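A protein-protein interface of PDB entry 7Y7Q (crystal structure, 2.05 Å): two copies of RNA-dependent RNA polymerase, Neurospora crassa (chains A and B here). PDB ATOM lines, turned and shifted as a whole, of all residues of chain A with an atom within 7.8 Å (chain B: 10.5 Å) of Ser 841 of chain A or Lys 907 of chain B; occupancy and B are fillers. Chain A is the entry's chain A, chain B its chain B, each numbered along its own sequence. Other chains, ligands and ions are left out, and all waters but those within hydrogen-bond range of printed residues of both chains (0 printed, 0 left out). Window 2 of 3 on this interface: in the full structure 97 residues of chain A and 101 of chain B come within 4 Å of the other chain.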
ATOM      1  N   PHE A 833      17.336  36.266  19.921  1.00  0.00           N
ATOM      2  CA  PHE A 833      16.861  34.944  19.450  1.00  0.00           C
ATOM      3  C   PHE A 833      17.552  34.575  18.137  1.00  0.00           C
ATOM      4  O   PHE A 833      18.177  33.514  18.072  1.00  0.00           O
ATOM      5  CB  PHE A 833      15.338  34.961  19.304  1.00  0.00           C
ATOM      6  CG  PHE A 833      14.742  33.780  18.582  1.00  0.00           C
ATOM      7  CD1 PHE A 833      14.527  32.583  19.241  1.00  0.00           C
ATOM      8  CD2 PHE A 833      14.384  33.870  17.248  1.00  0.00           C
ATOM      9  CE1 PHE A 833      13.981  31.498  18.578  1.00  0.00           C
ATOM     10  CE2 PHE A 833      13.836  32.786  16.587  1.00  0.00           C
ATOM     11  CZ  PHE A 833      13.636  31.602  17.254  1.00  0.00           C
ATOM     12  N   PHE A 834      17.435  35.421  17.120  1.00  0.00           N
ATOM     13  CA  PHE A 834      18.001  35.088  15.787  1.00  0.00           C
ATOM     14  C   PHE A 834      19.527  35.008  15.816  1.00  0.00           C
ATOM     15  O   PHE A 834      20.086  34.200  15.085  1.00  0.00           O
ATOM     16  CB  PHE A 834      17.477  35.983  14.668  1.00  0.00           C
ATOM     17  CG  PHE A 834      17.325  35.252  13.359  1.00  0.00           C
ATOM     18  CD1 PHE A 834      16.356  34.275  13.205  1.00  0.00           C
ATOM     19  CD2 PHE A 834      18.168  35.517  12.295  1.00  0.00           C
ATOM     20  CE1 PHE A 834      16.222  33.591  12.008  1.00  0.00           C
ATOM     21  CE2 PHE A 834      18.034  34.833  11.098  1.00  0.00           C
ATOM     22  CZ  PHE A 834      17.063  33.872  10.957  1.00  0.00           C
ATOM     23  N   LYS A 835      20.165  35.860  16.610  1.00  0.00           N
ATOM     24  CA  LYS A 835      21.643  35.855  16.691  1.00  0.00           C
ATOM     25  C   LYS A 835      22.090  34.477  17.181  1.00  0.00           C
ATOM     26  O   LYS A 835      23.062  33.959  16.636  1.00  0.00           O
ATOM     27  CB  LYS A 835      22.128  36.979  17.605  1.00  0.00           C
ATOM     28  CG  LYS A 835      23.603  37.333  17.493  1.00  0.00           C
ATOM     29  CD  LYS A 835      24.270  37.466  18.840  1.00  0.00           C
ATOM     30  CE  LYS A 835      25.713  37.909  18.739  1.00  0.00           C
ATOM     31  NZ  LYS A 835      26.646  36.776  18.945  1.00  0.00           N
ATOM     32  N   GLU A 836      21.371  33.901  18.141  1.00  0.00           N
ATOM     33  CA  GLU A 836      21.699  32.541  18.631  1.00  0.00           C
ATOM     34  C   GLU A 836      21.549  31.525  17.495  1.00  0.00           C
ATOM     35  O   GLU A 836      22.454  30.690  17.340  1.00  0.00           O
ATOM     36  CB  GLU A 836      20.806  32.183  19.816  1.00  0.00           C
ATOM     37  CG  GLU A 836      21.177  32.900  21.100  1.00  0.00           C
ATOM     38  CD  GLU A 836      20.046  33.043  22.106  1.00  0.00           C
ATOM     39  OE1 GLU A 836      20.282  33.622  23.183  1.00  0.00           O
ATOM     40  OE2 GLU A 836      18.931  32.574  21.810  1.00  0.00           O
ATOM     41  N   ILE A 837      20.474  31.618  16.710  1.00  0.00           N
ATOM     42  CA  ILE A 837      20.282  30.704  15.546  1.00  0.00           C
ATOM     43  C   ILE A 837      21.387  30.937  14.511  1.00  0.00           C
ATOM     44  O   ILE A 837      21.945  29.951  14.028  1.00  0.00           O
ATOM     45  CB  ILE A 837      18.883  30.908  14.939  1.00  0.00           C
ATOM     46  CG1 ILE A 837      17.783  30.783  15.993  1.00  0.00           C
ATOM     47  CG2 ILE A 837      18.652  29.969  13.766  1.00  0.00           C
ATOM     48  CD1 ILE A 837      16.815  29.661  15.736  1.00  0.00           C
ATOM     49  N   SER A 838      21.709  32.194  14.225  1.00  0.00           N
ATOM     50  CA  SER A 838      22.720  32.554  13.201  1.00  0.00           C
ATOM     51  C   SER A 838      24.102  32.048  13.621  1.00  0.00           C
ATOM     52  O   SER A 838      24.904  31.715  12.744  1.00  0.00           O
ATOM     53  CB  SER A 838      22.696  34.035  12.932  1.00  0.00           C
ATOM     54  OG  SER A 838      23.531  34.729  13.842  1.00  0.00           O
ATOM     55  N   ASP A 839      24.365  32.024  14.922  1.00  0.00           N
ATOM     56  CA  ASP A 839      25.669  31.552  15.446  1.00  0.00           C
ATOM     57  C   ASP A 839      25.877  30.084  15.051  1.00  0.00           C
ATOM     58  O   ASP A 839      27.031  29.708  14.810  1.00  0.00           O
ATOM     59  CB  ASP A 839      25.768  31.807  16.948  1.00  0.00           C
ATOM     60  CG  ASP A 839      26.083  33.252  17.293  1.00  0.00           C
ATOM     61  OD1 ASP A 839      26.485  33.996  16.382  1.00  0.00           O
ATOM     62  OD2 ASP A 839      25.919  33.619  18.467  1.00  0.00           O
ATOM     63  N   LYS A 840      24.809  29.285  15.035  1.00  0.00           N
ATOM     64  CA  LYS A 840      24.915  27.856  14.649  1.00  0.00           C
ATOM     65  C   LYS A 840      24.398  27.569  13.228  1.00  0.00           C
ATOM     66  O   LYS A 840      24.333  26.383  12.879  1.00  0.00           O
ATOM     67  CB  LYS A 840      24.159  27.001  15.668  1.00  0.00           C
ATOM     68  N   SER A 841      24.006  28.579  12.451  1.00  0.00           N
ATOM     69  CA  SER A 841      23.587  28.322  11.045  1.00  0.00           C
ATOM     70  C   SER A 841      24.167  29.364  10.092  1.00  0.00           C
ATOM     71  O   SER A 841      24.011  30.557  10.362  1.00  0.00           O
ATOM     72  CB  SER A 841      22.093  28.235  10.905  1.00  0.00           C
ATOM     73  OG  SER A 841      21.694  28.435   9.560  1.00  0.00           O
ATOM     74  N   ARG A 842      24.727  28.918   8.969  1.00  0.00           N
ATOM     75  CA  ARG A 842      25.384  29.851   8.018  1.00  0.00           C
ATOM     76  C   ARG A 842      24.324  30.523   7.157  1.00  0.00           C
ATOM     77  O   ARG A 842      24.513  31.690   6.796  1.00  0.00           O
ATOM     78  N   SER A 843      23.263  29.788   6.841  1.00  0.00           N
ATOM     79  CA  SER A 843      22.158  30.363   6.036  1.00  0.00           C
ATOM     80  C   SER A 843      21.467  31.461   6.845  1.00  0.00           C
ATOM     81  O   SER A 843      21.183  32.521   6.276  1.00  0.00           O
ATOM     82  CB  SER A 843      21.194  29.292   5.632  1.00  0.00           C
ATOM     83  OG  SER A 843      20.622  28.670   6.771  1.00  0.00           O
ATOM     84  N   SER A 844      21.257  31.211   8.137  1.00  0.00           N
ATOM     85  CA  SER A 844      20.587  32.193   9.020  1.00  0.00           C
ATOM     86  C   SER A 844      21.505  33.392   9.237  1.00  0.00           C
ATOM     87  O   SER A 844      20.990  34.498   9.353  1.00  0.00           O
ATOM     88  CB  SER A 844      20.217  31.542  10.305  1.00  0.00           C
ATOM     89  OG  SER A 844      19.159  30.626  10.100  1.00  0.00           O
ATOM     90  N   ALA A 845      22.816  33.157   9.279  1.00  0.00           N
ATOM     91  CA  ALA A 845      23.787  34.259   9.433  1.00  0.00           C
ATOM     92  C   ALA A 845      23.803  35.148   8.195  1.00  0.00           C
ATOM     93  O   ALA A 845      23.939  36.356   8.361  1.00  0.00           O
ATOM     94  CB  ALA A 845      25.145  33.725   9.765  1.00  0.00           C
ATOM     95  N   LEU A 846      23.692  34.568   7.003  1.00  0.00           N
ATOM     96  CA  LEU A 846      23.616  35.397   5.768  1.00  0.00           C
ATOM     97  C   LEU A 846      22.339  36.241   5.768  1.00  0.00           C
ATOM     98  O   LEU A 846      22.420  37.424   5.435  1.00  0.00           O
ATOM     99  CB  LEU A 846      23.672  34.483   4.541  1.00  0.00           C
ATOM    100  CG  LEU A 846      24.072  35.160   3.233  1.00  0.00           C
ATOM    101  CD1 LEU A 846      25.377  35.922   3.397  1.00  0.00           C
ATOM    102  CD2 LEU A 846      24.188  34.140   2.114  1.00  0.00           C
ATOM    103  N   LEU A 847      21.215  35.637   6.146  1.00  0.00           N
ATOM    104  CA  LEU A 847      19.932  36.372   6.210  1.00  0.00           C
ATOM    105  C   LEU A 847      20.095  37.430   7.285  1.00  0.00           C
ATOM    106  O   LEU A 847      19.733  38.581   7.043  1.00  0.00           O
ATOM    107  CB  LEU A 847      18.837  35.385   6.604  1.00  0.00           C
ATOM    108  CG  LEU A 847      17.420  35.942   6.674  1.00  0.00           C
ATOM    109  CD1 LEU A 847      16.943  36.364   5.296  1.00  0.00           C
ATOM    110  CD2 LEU A 847      16.477  34.909   7.268  1.00  0.00           C
ATOM    111  N   PHE A 848      20.676  37.028   8.413  1.00  0.00           N
ATOM    112  CA  PHE A 848      20.779  37.988   9.507  1.00  0.00           C
ATOM    113  C   PHE A 848      21.692  39.152   9.139  1.00  0.00           C
ATOM    114  O   PHE A 848      21.418  40.303   9.500  1.00  0.00           O
ATOM    115  CB  PHE A 848      21.279  37.274  10.763  1.00  0.00           C
ATOM    116  CG  PHE A 848      21.091  38.056  12.031  1.00  0.00           C
ATOM    117  CD1 PHE A 848      20.039  38.946  12.167  1.00  0.00           C
ATOM    118  CD2 PHE A 848      21.953  37.876  13.101  1.00  0.00           C
ATOM    119  CE1 PHE A 848      19.864  39.659  13.341  1.00  0.00           C
ATOM    120  CE2 PHE A 848      21.783  38.582  14.274  1.00  0.00           C
ATOM    121  CZ  PHE A 848      20.738  39.475  14.397  1.00  0.00           C
ATOM    122  N   SER A 906      14.298  27.243   3.739  1.00  0.00           N
ATOM    123  CA  SER A 906      13.063  27.909   3.253  1.00  0.00           C
ATOM    124  C   SER A 906      11.965  27.763   4.302  1.00  0.00           C
ATOM    125  O   SER A 906      11.062  28.602   4.313  1.00  0.00           O
ATOM    126  CB  SER A 906      12.623  27.381   1.913  1.00  0.00           C
ATOM    127  OG  SER A 906      12.192  28.437   1.071  1.00  0.00           O
ATOM    128  N   LYS A 907      12.050  26.740   5.149  1.00  0.00           N
ATOM    129  CA  LYS A 907      11.068  26.588   6.246  1.00  0.00           C
ATOM    130  C   LYS A 907      11.206  27.796   7.184  1.00  0.00           C
ATOM    131  O   LYS A 907      10.177  28.327   7.599  1.00  0.00           O
ATOM    132  CB  LYS A 907      11.279  25.242   6.939  1.00  0.00           C
ATOM    133  CG  LYS A 907      10.864  24.016   6.140  1.00  0.00           C
ATOM    134  CD  LYS A 907      10.869  22.747   6.958  1.00  0.00           C
ATOM    135  CE  LYS A 907      12.258  22.332   7.393  1.00  0.00           C
ATOM    136  NZ  LYS A 907      13.257  22.549   6.321  1.00  0.00           N
ATOM    137  N   VAL A 908      12.438  28.228   7.463  1.00  0.00           N
ATOM    138  CA  VAL A 908      12.660  29.443   8.300  1.00  0.00           C
ATOM    139  C   VAL A 908      12.089  30.671   7.582  1.00  0.00           C
ATOM    140  O   VAL A 908      11.389  31.455   8.222  1.00  0.00           O
ATOM    141  CB  VAL A 908      14.151  29.625   8.639  1.00  0.00           C
ATOM    142  CG1 VAL A 908      14.460  31.007   9.191  1.00  0.00           C
ATOM    143  CG2 VAL A 908      14.643  28.543   9.583  1.00  0.00           C
ATOM    144  N   LEU A 911       8.317  30.592   7.785  1.00  0.00           N
ATOM    145  CA  LEU A 911       7.813  30.856   9.150  1.00  0.00           C
ATOM    146  C   LEU A 911       7.992  32.337   9.488  1.00  0.00           C
ATOM    147  O   LEU A 911       7.171  32.864  10.226  1.00  0.00           O
ATOM    148  CB  LEU A 911       8.560  29.946  10.123  1.00  0.00           C
ATOM    149  CG  LEU A 911       7.833  28.666  10.520  1.00  0.00           C
ATOM    150  CD1 LEU A 911       8.810  27.650  11.084  1.00  0.00           C
ATOM    151  CD2 LEU A 911       6.735  28.966  11.525  1.00  0.00           C
ATOM    152  N   PHE B 834       1.049  25.174   7.805  1.00  0.00           N
ATOM    153  CA  PHE B 834       1.946  24.062   8.212  1.00  0.00           C
ATOM    154  C   PHE B 834       1.726  22.811   7.363  1.00  0.00           C
ATOM    155  O   PHE B 834       2.669  22.047   7.216  1.00  0.00           O
ATOM    156  CB  PHE B 834       1.912  23.824   9.724  1.00  0.00           C
ATOM    157  CG  PHE B 834       3.231  23.386  10.300  1.00  0.00           C
ATOM    158  CD1 PHE B 834       4.298  24.265  10.372  1.00  0.00           C
ATOM    159  CD2 PHE B 834       3.413  22.090  10.749  1.00  0.00           C
ATOM    160  CE1 PHE B 834       5.516  23.860  10.888  1.00  0.00           C
ATOM    161  CE2 PHE B 834       4.631  21.686  11.270  1.00  0.00           C
ATOM    162  CZ  PHE B 834       5.680  22.571  11.338  1.00  0.00           C
ATOM    163  N   ILE B 837       3.922  22.869   4.489  1.00  0.00           N
ATOM    164  CA  ILE B 837       5.304  22.592   4.974  1.00  0.00           C
ATOM    165  C   ILE B 837       5.411  21.095   5.267  1.00  0.00           C
ATOM    166  O   ILE B 837       6.424  20.499   4.885  1.00  0.00           O
ATOM    167  CB  ILE B 837       5.593  23.447   6.222  1.00  0.00           C
ATOM    168  CG1 ILE B 837       5.555  24.943   5.907  1.00  0.00           C
ATOM    169  CG2 ILE B 837       6.904  23.047   6.876  1.00  0.00           C
ATOM    170  CD1 ILE B 837       6.358  25.778   6.869  1.00  0.00           C
ATOM    171  N   SER B 843       9.891  15.412   8.973  1.00  0.00           N
ATOM    172  CA  SER B 843      10.028  15.869  10.377  1.00  0.00           C
ATOM    173  C   SER B 843       8.845  16.762  10.737  1.00  0.00           C
ATOM    174  O   SER B 843       8.280  16.578  11.824  1.00  0.00           O
ATOM    175  CB  SER B 843      11.305  16.624  10.542  1.00  0.00           C
ATOM    176  OG  SER B 843      11.533  17.480   9.434  1.00  0.00           O
ATOM    177  N   SER B 844       8.497  17.683   9.844  1.00  0.00           N
ATOM    178  CA  SER B 844       7.346  18.585  10.078  1.00  0.00           C
ATOM    179  C   SER B 844       6.056  17.769  10.113  1.00  0.00           C
ATOM    180  O   SER B 844       5.219  18.060  10.955  1.00  0.00           O
ATOM    181  CB  SER B 844       7.308  19.682   9.057  1.00  0.00           C
ATOM    182  OG  SER B 844       8.551  20.361   8.999  1.00  0.00           O
ATOM    183  N   LEU B 847       5.815  16.107  13.409  1.00  0.00           N
ATOM    184  CA  LEU B 847       5.471  17.110  14.442  1.00  0.00           C
ATOM    185  C   LEU B 847       4.004  17.447  14.246  1.00  0.00           C
ATOM    186  O   LEU B 847       3.271  17.526  15.234  1.00  0.00           O
ATOM    187  CB  LEU B 847       6.337  18.353  14.218  1.00  0.00           C
ATOM    188  CG  LEU B 847       6.115  19.509  15.187  1.00  0.00           C
ATOM    189  CD1 LEU B 847       6.585  19.138  16.584  1.00  0.00           C
ATOM    190  CD2 LEU B 847       6.833  20.756  14.700  1.00  0.00           C
ATOM    191  N   PRO B 894       5.755  21.514  21.533  1.00  0.00           N
ATOM    192  CA  PRO B 894       6.559  20.937  20.473  1.00  0.00           C
ATOM    193  C   PRO B 894       7.464  19.788  20.941  1.00  0.00           C
ATOM    194  O   PRO B 894       7.974  19.871  22.041  1.00  0.00           O
ATOM    195  CB  PRO B 894       7.410  22.126  20.041  1.00  0.00           C
ATOM    196  CG  PRO B 894       6.570  23.325  20.350  1.00  0.00           C
ATOM    197  CD  PRO B 894       5.911  22.961  21.658  1.00  0.00           C
ATOM    198  N   SER B 906      16.228  22.035  16.492  1.00  0.00           N
ATOM    199  CA  SER B 906      15.735  22.409  15.172  1.00  0.00           C
ATOM    200  C   SER B 906      15.388  23.892  15.111  1.00  0.00           C
ATOM    201  O   SER B 906      14.957  24.481  16.103  1.00  0.00           O
ATOM    202  CB  SER B 906      14.510  21.571  14.798  1.00  0.00           C
ATOM    203  OG  SER B 906      14.078  21.858  13.479  1.00  0.00           O
ATOM    204  N   LYS B 907      15.567  24.484  13.934  1.00  0.00           N
ATOM    205  CA  LYS B 907      15.233  25.911  13.759  1.00  0.00           C
ATOM    206  C   LYS B 907      13.708  26.086  13.765  1.00  0.00           C
ATOM    207  O   LYS B 907      13.257  27.148  14.192  1.00  0.00           O
ATOM    208  CB  LYS B 907      15.894  26.456  12.494  1.00  0.00           C
ATOM    209  CG  LYS B 907      17.391  26.217  12.379  1.00  0.00           C
ATOM    210  CD  LYS B 907      17.795  25.638  11.042  1.00  0.00           C
ATOM    211  CE  LYS B 907      17.958  26.691   9.968  1.00  0.00           C
ATOM    212  NZ  LYS B 907      18.557  27.931  10.511  1.00  0.00           N
ATOM    213  N   VAL B 908      12.957  25.074  13.333  1.00  0.00           N
ATOM    214  CA  VAL B 908      11.502  25.183  13.317  1.00  0.00           C
ATOM    215  C   VAL B 908      10.952  25.167  14.740  1.00  0.00           C
ATOM    216  O   VAL B 908      10.130  26.011  15.115  1.00  0.00           O
ATOM    217  CB  VAL B 908      10.887  24.062  12.461  1.00  0.00           C
ATOM    218  CG1 VAL B 908       9.424  23.852  12.828  1.00  0.00           C
ATOM    219  CG2 VAL B 908      11.031  24.382  10.980  1.00  0.00           C
ATOM    220  N   ILE B 909      11.397  24.204  15.550  1.00  0.00           N
ATOM    221  CA  ILE B 909      10.935  24.125  16.932  1.00  0.00           C
ATOM    222  C   ILE B 909      11.232  25.426  17.666  1.00  0.00           C
ATOM    223  O   ILE B 909      10.414  25.912  18.458  1.00  0.00           O
ATOM    224  CB  ILE B 909      11.574  22.920  17.643  1.00  0.00           C
ATOM    225  CG1 ILE B 909      10.931  21.615  17.172  1.00  0.00           C
ATOM    226  CG2 ILE B 909      11.435  23.062  19.150  1.00  0.00           C
ATOM    227  CD1 ILE B 909       9.520  21.415  17.669  1.00  0.00           C
ATOM    228  N   ARG B 910      12.384  26.026  17.385  1.00  0.00           N
ATOM    229  CA  ARG B 910      12.772  27.281  18.082  1.00  0.00           C
ATOM    230  C   ARG B 910      11.863  28.433  17.645  1.00  0.00           C
ATOM    231  O   ARG B 910      11.445  29.211  18.504  1.00  0.00           O
ATOM    232  CB  ARG B 910      14.249  27.608  17.845  1.00  0.00           C
ATOM    233  CG  ARG B 910      15.191  27.054  18.904  1.00  0.00           C
ATOM    234  CD  ARG B 910      16.579  26.801  18.352  1.00  0.00           C
ATOM    235  NE  ARG B 910      17.540  26.381  19.361  1.00  0.00           N
ATOM    236  CZ  ARG B 910      18.645  27.048  19.681  1.00  0.00           C
ATOM    237  NH1 ARG B 910      18.939  28.185  19.074  1.00  0.00           N
ATOM    238  NH2 ARG B 910      19.453  26.576  20.611  1.00  0.00           N
ATOM    239  N   LEU B 911      11.594  28.535  16.350  1.00  0.00           N
ATOM    240  CA  LEU B 911      10.735  29.620  15.819  1.00  0.00           C
ATOM    241  C   LEU B 911       9.311  29.486  16.368  1.00  0.00           C
ATOM    242  O   LEU B 911       8.718  30.507  16.690  1.00  0.00           O
ATOM    243  CB  LEU B 911      10.777  29.575  14.293  1.00  0.00           C
ATOM    244  CG  LEU B 911      11.882  30.409  13.653  1.00  0.00           C
ATOM    245  CD1 LEU B 911      12.095  30.005  12.207  1.00  0.00           C
ATOM    246  CD2 LEU B 911      11.562  31.889  13.750  1.00  0.00           C
ATOM    247  N   LEU B 912       8.785  28.272  16.440  1.00  0.00           N
ATOM    248  CA  LEU B 912       7.431  28.038  16.994  1.00  0.00           C
ATOM    249  C   LEU B 912       7.378  28.327  18.496  1.00  0.00           C
ATOM    250  O   LEU B 912       6.401  28.926  18.931  1.00  0.00           O
ATOM    251  CB  LEU B 912       7.070  26.580  16.705  1.00  0.00           C
ATOM    252  CG  LEU B 912       6.682  26.272  15.261  1.00  0.00           C
ATOM    253  CD1 LEU B 912       6.504  24.779  15.057  1.00  0.00           C
ATOM    254  CD2 LEU B 912       5.416  27.014  14.872  1.00  0.00           C
ATOM    255  N   GLU B 913       8.374  27.868  19.248  1.00  0.00           N
ATOM    256  CA  GLU B 913       8.388  28.016  20.731  1.00  0.00           C
ATOM    257  C   GLU B 913       8.611  29.454  21.209  1.00  0.00           C
ATOM    258  O   GLU B 913       8.027  29.798  22.230  1.00  0.00           O
ATOM    259  CB  GLU B 913       9.402  27.059  21.357  1.00  0.00           C
ATOM    260  CG  GLU B 913       8.798  25.770  21.872  1.00  0.00           C
ATOM    261  CD  GLU B 913       9.825  24.701  22.206  1.00  0.00           C
ATOM    262  OE1 GLU B 913       9.438  23.527  22.330  1.00  0.00           O
ATOM    263  OE2 GLU B 913      11.010  25.048  22.344  1.00  0.00           O
ATOM    264  N   LEU B 914       9.484  30.218  20.552  1.00  0.00           N
ATOM    265  CA  LEU B 914       9.855  31.574  21.036  1.00  0.00           C
ATOM    266  C   LEU B 914      10.044  31.474  22.552  1.00  0.00           C
ATOM    267  O   LEU B 914       9.297  32.147  23.276  1.00  0.00           O
ATOM    268  CB  LEU B 914       8.774  32.570  20.619  1.00  0.00           C
ATOM    269  CG  LEU B 914       8.494  32.646  19.120  1.00  0.00           C
ATOM    270  CD1 LEU B 914       7.289  33.526  18.840  1.00  0.00           C
ATOM    271  CD2 LEU B 914       9.713  33.152  18.369  1.00  0.00           C
ATOM    272  N   SER B 915      11.026  30.697  23.004  1.00  0.00           N
ATOM    273  CA  SER B 915      11.226  30.404  24.450  1.00  0.00           C
ATOM    274  C   SER B 915      11.544  31.652  25.279  1.00  0.00           C
ATOM    275  O   SER B 915      11.317  31.612  26.489  1.00  0.00           O
ATOM    276  CB  SER B 915      12.273  29.335  24.617  1.00  0.00           C
ATOM    277  OG  SER B 915      11.820  28.097  24.099  1.00  0.00           O
ATOM    278  N   PHE B 916      12.067  32.698  24.650  1.00  0.00           N
ATOM    279  CA  PHE B 916      12.363  33.976  25.338  1.00  0.00           C
ATOM    280  C   PHE B 916      11.068  34.567  25.894  1.00  0.00           C
ATOM    281  O   PHE B 916      11.137  35.385  26.807  1.00  0.00           O
ATOM    282  CB  PHE B 916      13.065  34.941  24.385  1.00  0.00           C
ATOM    283  CG  PHE B 916      12.335  35.268  23.108  1.00  0.00           C
ATOM    284  CD1 PHE B 916      12.466  34.465  21.990  1.00  0.00           C
ATOM    285  CD2 PHE B 916      11.539  36.397  23.018  1.00  0.00           C
ATOM    286  CE1 PHE B 916      11.804  34.774  20.812  1.00  0.00           C
ATOM    287  CE2 PHE B 916      10.879  36.706  21.841  1.00  0.00           C
ATOM    288  CZ  PHE B 916      11.014  35.895  20.742  1.00  0.00           C
ATOM    289  N   THR B 924       4.022  31.216  18.566  1.00  0.00           N
ATOM    290  CA  THR B 924       3.449  30.797  17.262  1.00  0.00           C
ATOM    291  C   THR B 924       2.861  29.383  17.361  1.00  0.00           C
ATOM    292  O   THR B 924       1.914  29.101  16.634  1.00  0.00           O
ATOM    293  CB  THR B 924       4.487  30.989  16.155  1.00  0.00           C
ATOM    294  OG1 THR B 924       4.948  32.333  16.253  1.00  0.00           O
ATOM    295  CG2 THR B 924       3.930  30.735  14.773  1.00  0.00           C
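The side-chain hydroxyl of Ser 906 of chain B lies close to the backbone NH of Val 908 of chain B, 3.4 Å away.
The side-chain hydroxyl (OG) of Ser 841 of chain A lies within hydrogen-bond range of the backbone NH (N) of Ser 844 of chain A (3.1 Å).
OG of Ser 843 of chain A sits at hydrogen-bond distance from OG of Ser 841 of chain A (3.0 Å).
NZ of Lys 907 of chain B sits at hydrogen-bond distance from OG of Ser 844 of chain A, 2.8 Å away.
The side-chain hydroxyl of Ser 841 of chain A is in hydrogen-bond range of the side-chain amino group of Lys 907 of chain B (3.3 Å).
Arg 910 of chain B touches Phe 833 of chain A (O to CE1, 3.4 Å).
Phe 833 of chain A touches Leu 911 of chain B (CE2 to CD2, 3.7 Å).
Phe 833 of chain A touches Phe 916 of chain B (CG to CE1, 3.8 Å).
Lys 907 of chain B touches Ile 837 of chain A.
Ile 837 of chain A touches Arg 910 of chain B.
Lys 907 of chain A touches Ile 837 of chain B (CD to CG2, 3.98 Å).
Lys 907 of chain A touches Ser 844 of chain B.
Lys 907 of chain B touches Val 908 of chain A.
CG2 of Val 908 of chain A touches CD1 of Leu 911 of chain B, at 3.9 Å.
CD1 of Leu 911 of chain A touches CG2 of Val 908 of chain B (3.95 Å).
Ile 837 of chain A touches Lys 907 of chain B, and with the chains exchanged Lys 907 of chain A touches Ile 837 of chain B.
Ser 844 of chain A touches Lys 907 of chain B, and with the chains exchanged Lys 907 of chain A touches Ser 844 of chain B.
Val 908 of chain A touches Lys 907 of chain B, but with the chains exchanged Lys 907 of chain A does not touch Val 908 of chain B (4.1 Å).
Val 908 of chain A touches Leu 911 of chain B, and with the chains exchanged Leu 911 of chain A touches Val 908 of chain B.
Positions printed for both chains: 834, 837, 843, 844, 847, 906, 907, 908 and 911.
Of the 12 pairs that touch across the chains among the printed residues, 6 have their exchanged pair printed and touching as well.
Of chain B, only Lys 907 (3.3 Å) comes within 4 Å of Ser 841 of chain A.
Lys 907 of chain B touches four residues of chain A.
Ile 837 of chain A touches just these residues of chain B: Lys 907 and Arg 910.
No residue of chain B comes within 4 Å of Ser 838 of chain A.
No residue of chain B comes within 4 Å of Lys 840 of chain A.
No residue of chain B comes within 4 Å of Ser 843 of chain A.
Of chain B, only Lys 907 comes within 4 Å of Ser 844 of chain A.
No residue of chain B comes within 4 Å of Ala 845 of chain A.
Printed residues of chain A within 4 Å of Phe 916 of chain B: Phe 833.
Of the printed residues of chain A, Val 908 of chain B touches Leu 911 (3.95 Å).
Of the printed residues of chain B, Leu 911 of chain A touches Val 908.
Of the printed residues of chain B, Lys 907 of chain A touches Ile 837 and Ser 844.
Printed residues of chain A within 4 Å of Leu 911 of chain B: Phe 833 (3.7 Å) and Val 908 (3.9 Å).
Leu 847 of chain B touches none of the printed residues of chain A.
Asp 839 of chain A touches none of the printed residues of chain B.
The nearest printed residue of chain A that does not touch Leu 911 of chain B is Leu 911 of chain A (4.1 Å).
Of the 18 printed residues of chain B, 7 touch a printed residue of chain A.
Printed residues of chain A that touch a printed residue of chain B: Phe 833, Ile 837, Ser 841, Ser 844, Lys 907, Val 908 and Leu 911.
Hydrophobic or aromatic side chains of chain A within 4 Å of the printed part of chain B: Phe 833, Ile 837, Val 908 and Leu 911.
Among the printed residues, no Asp or Glu carboxylate lies within 4 Å of a Lys or Arg side-chain nitrogen of the other chain.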
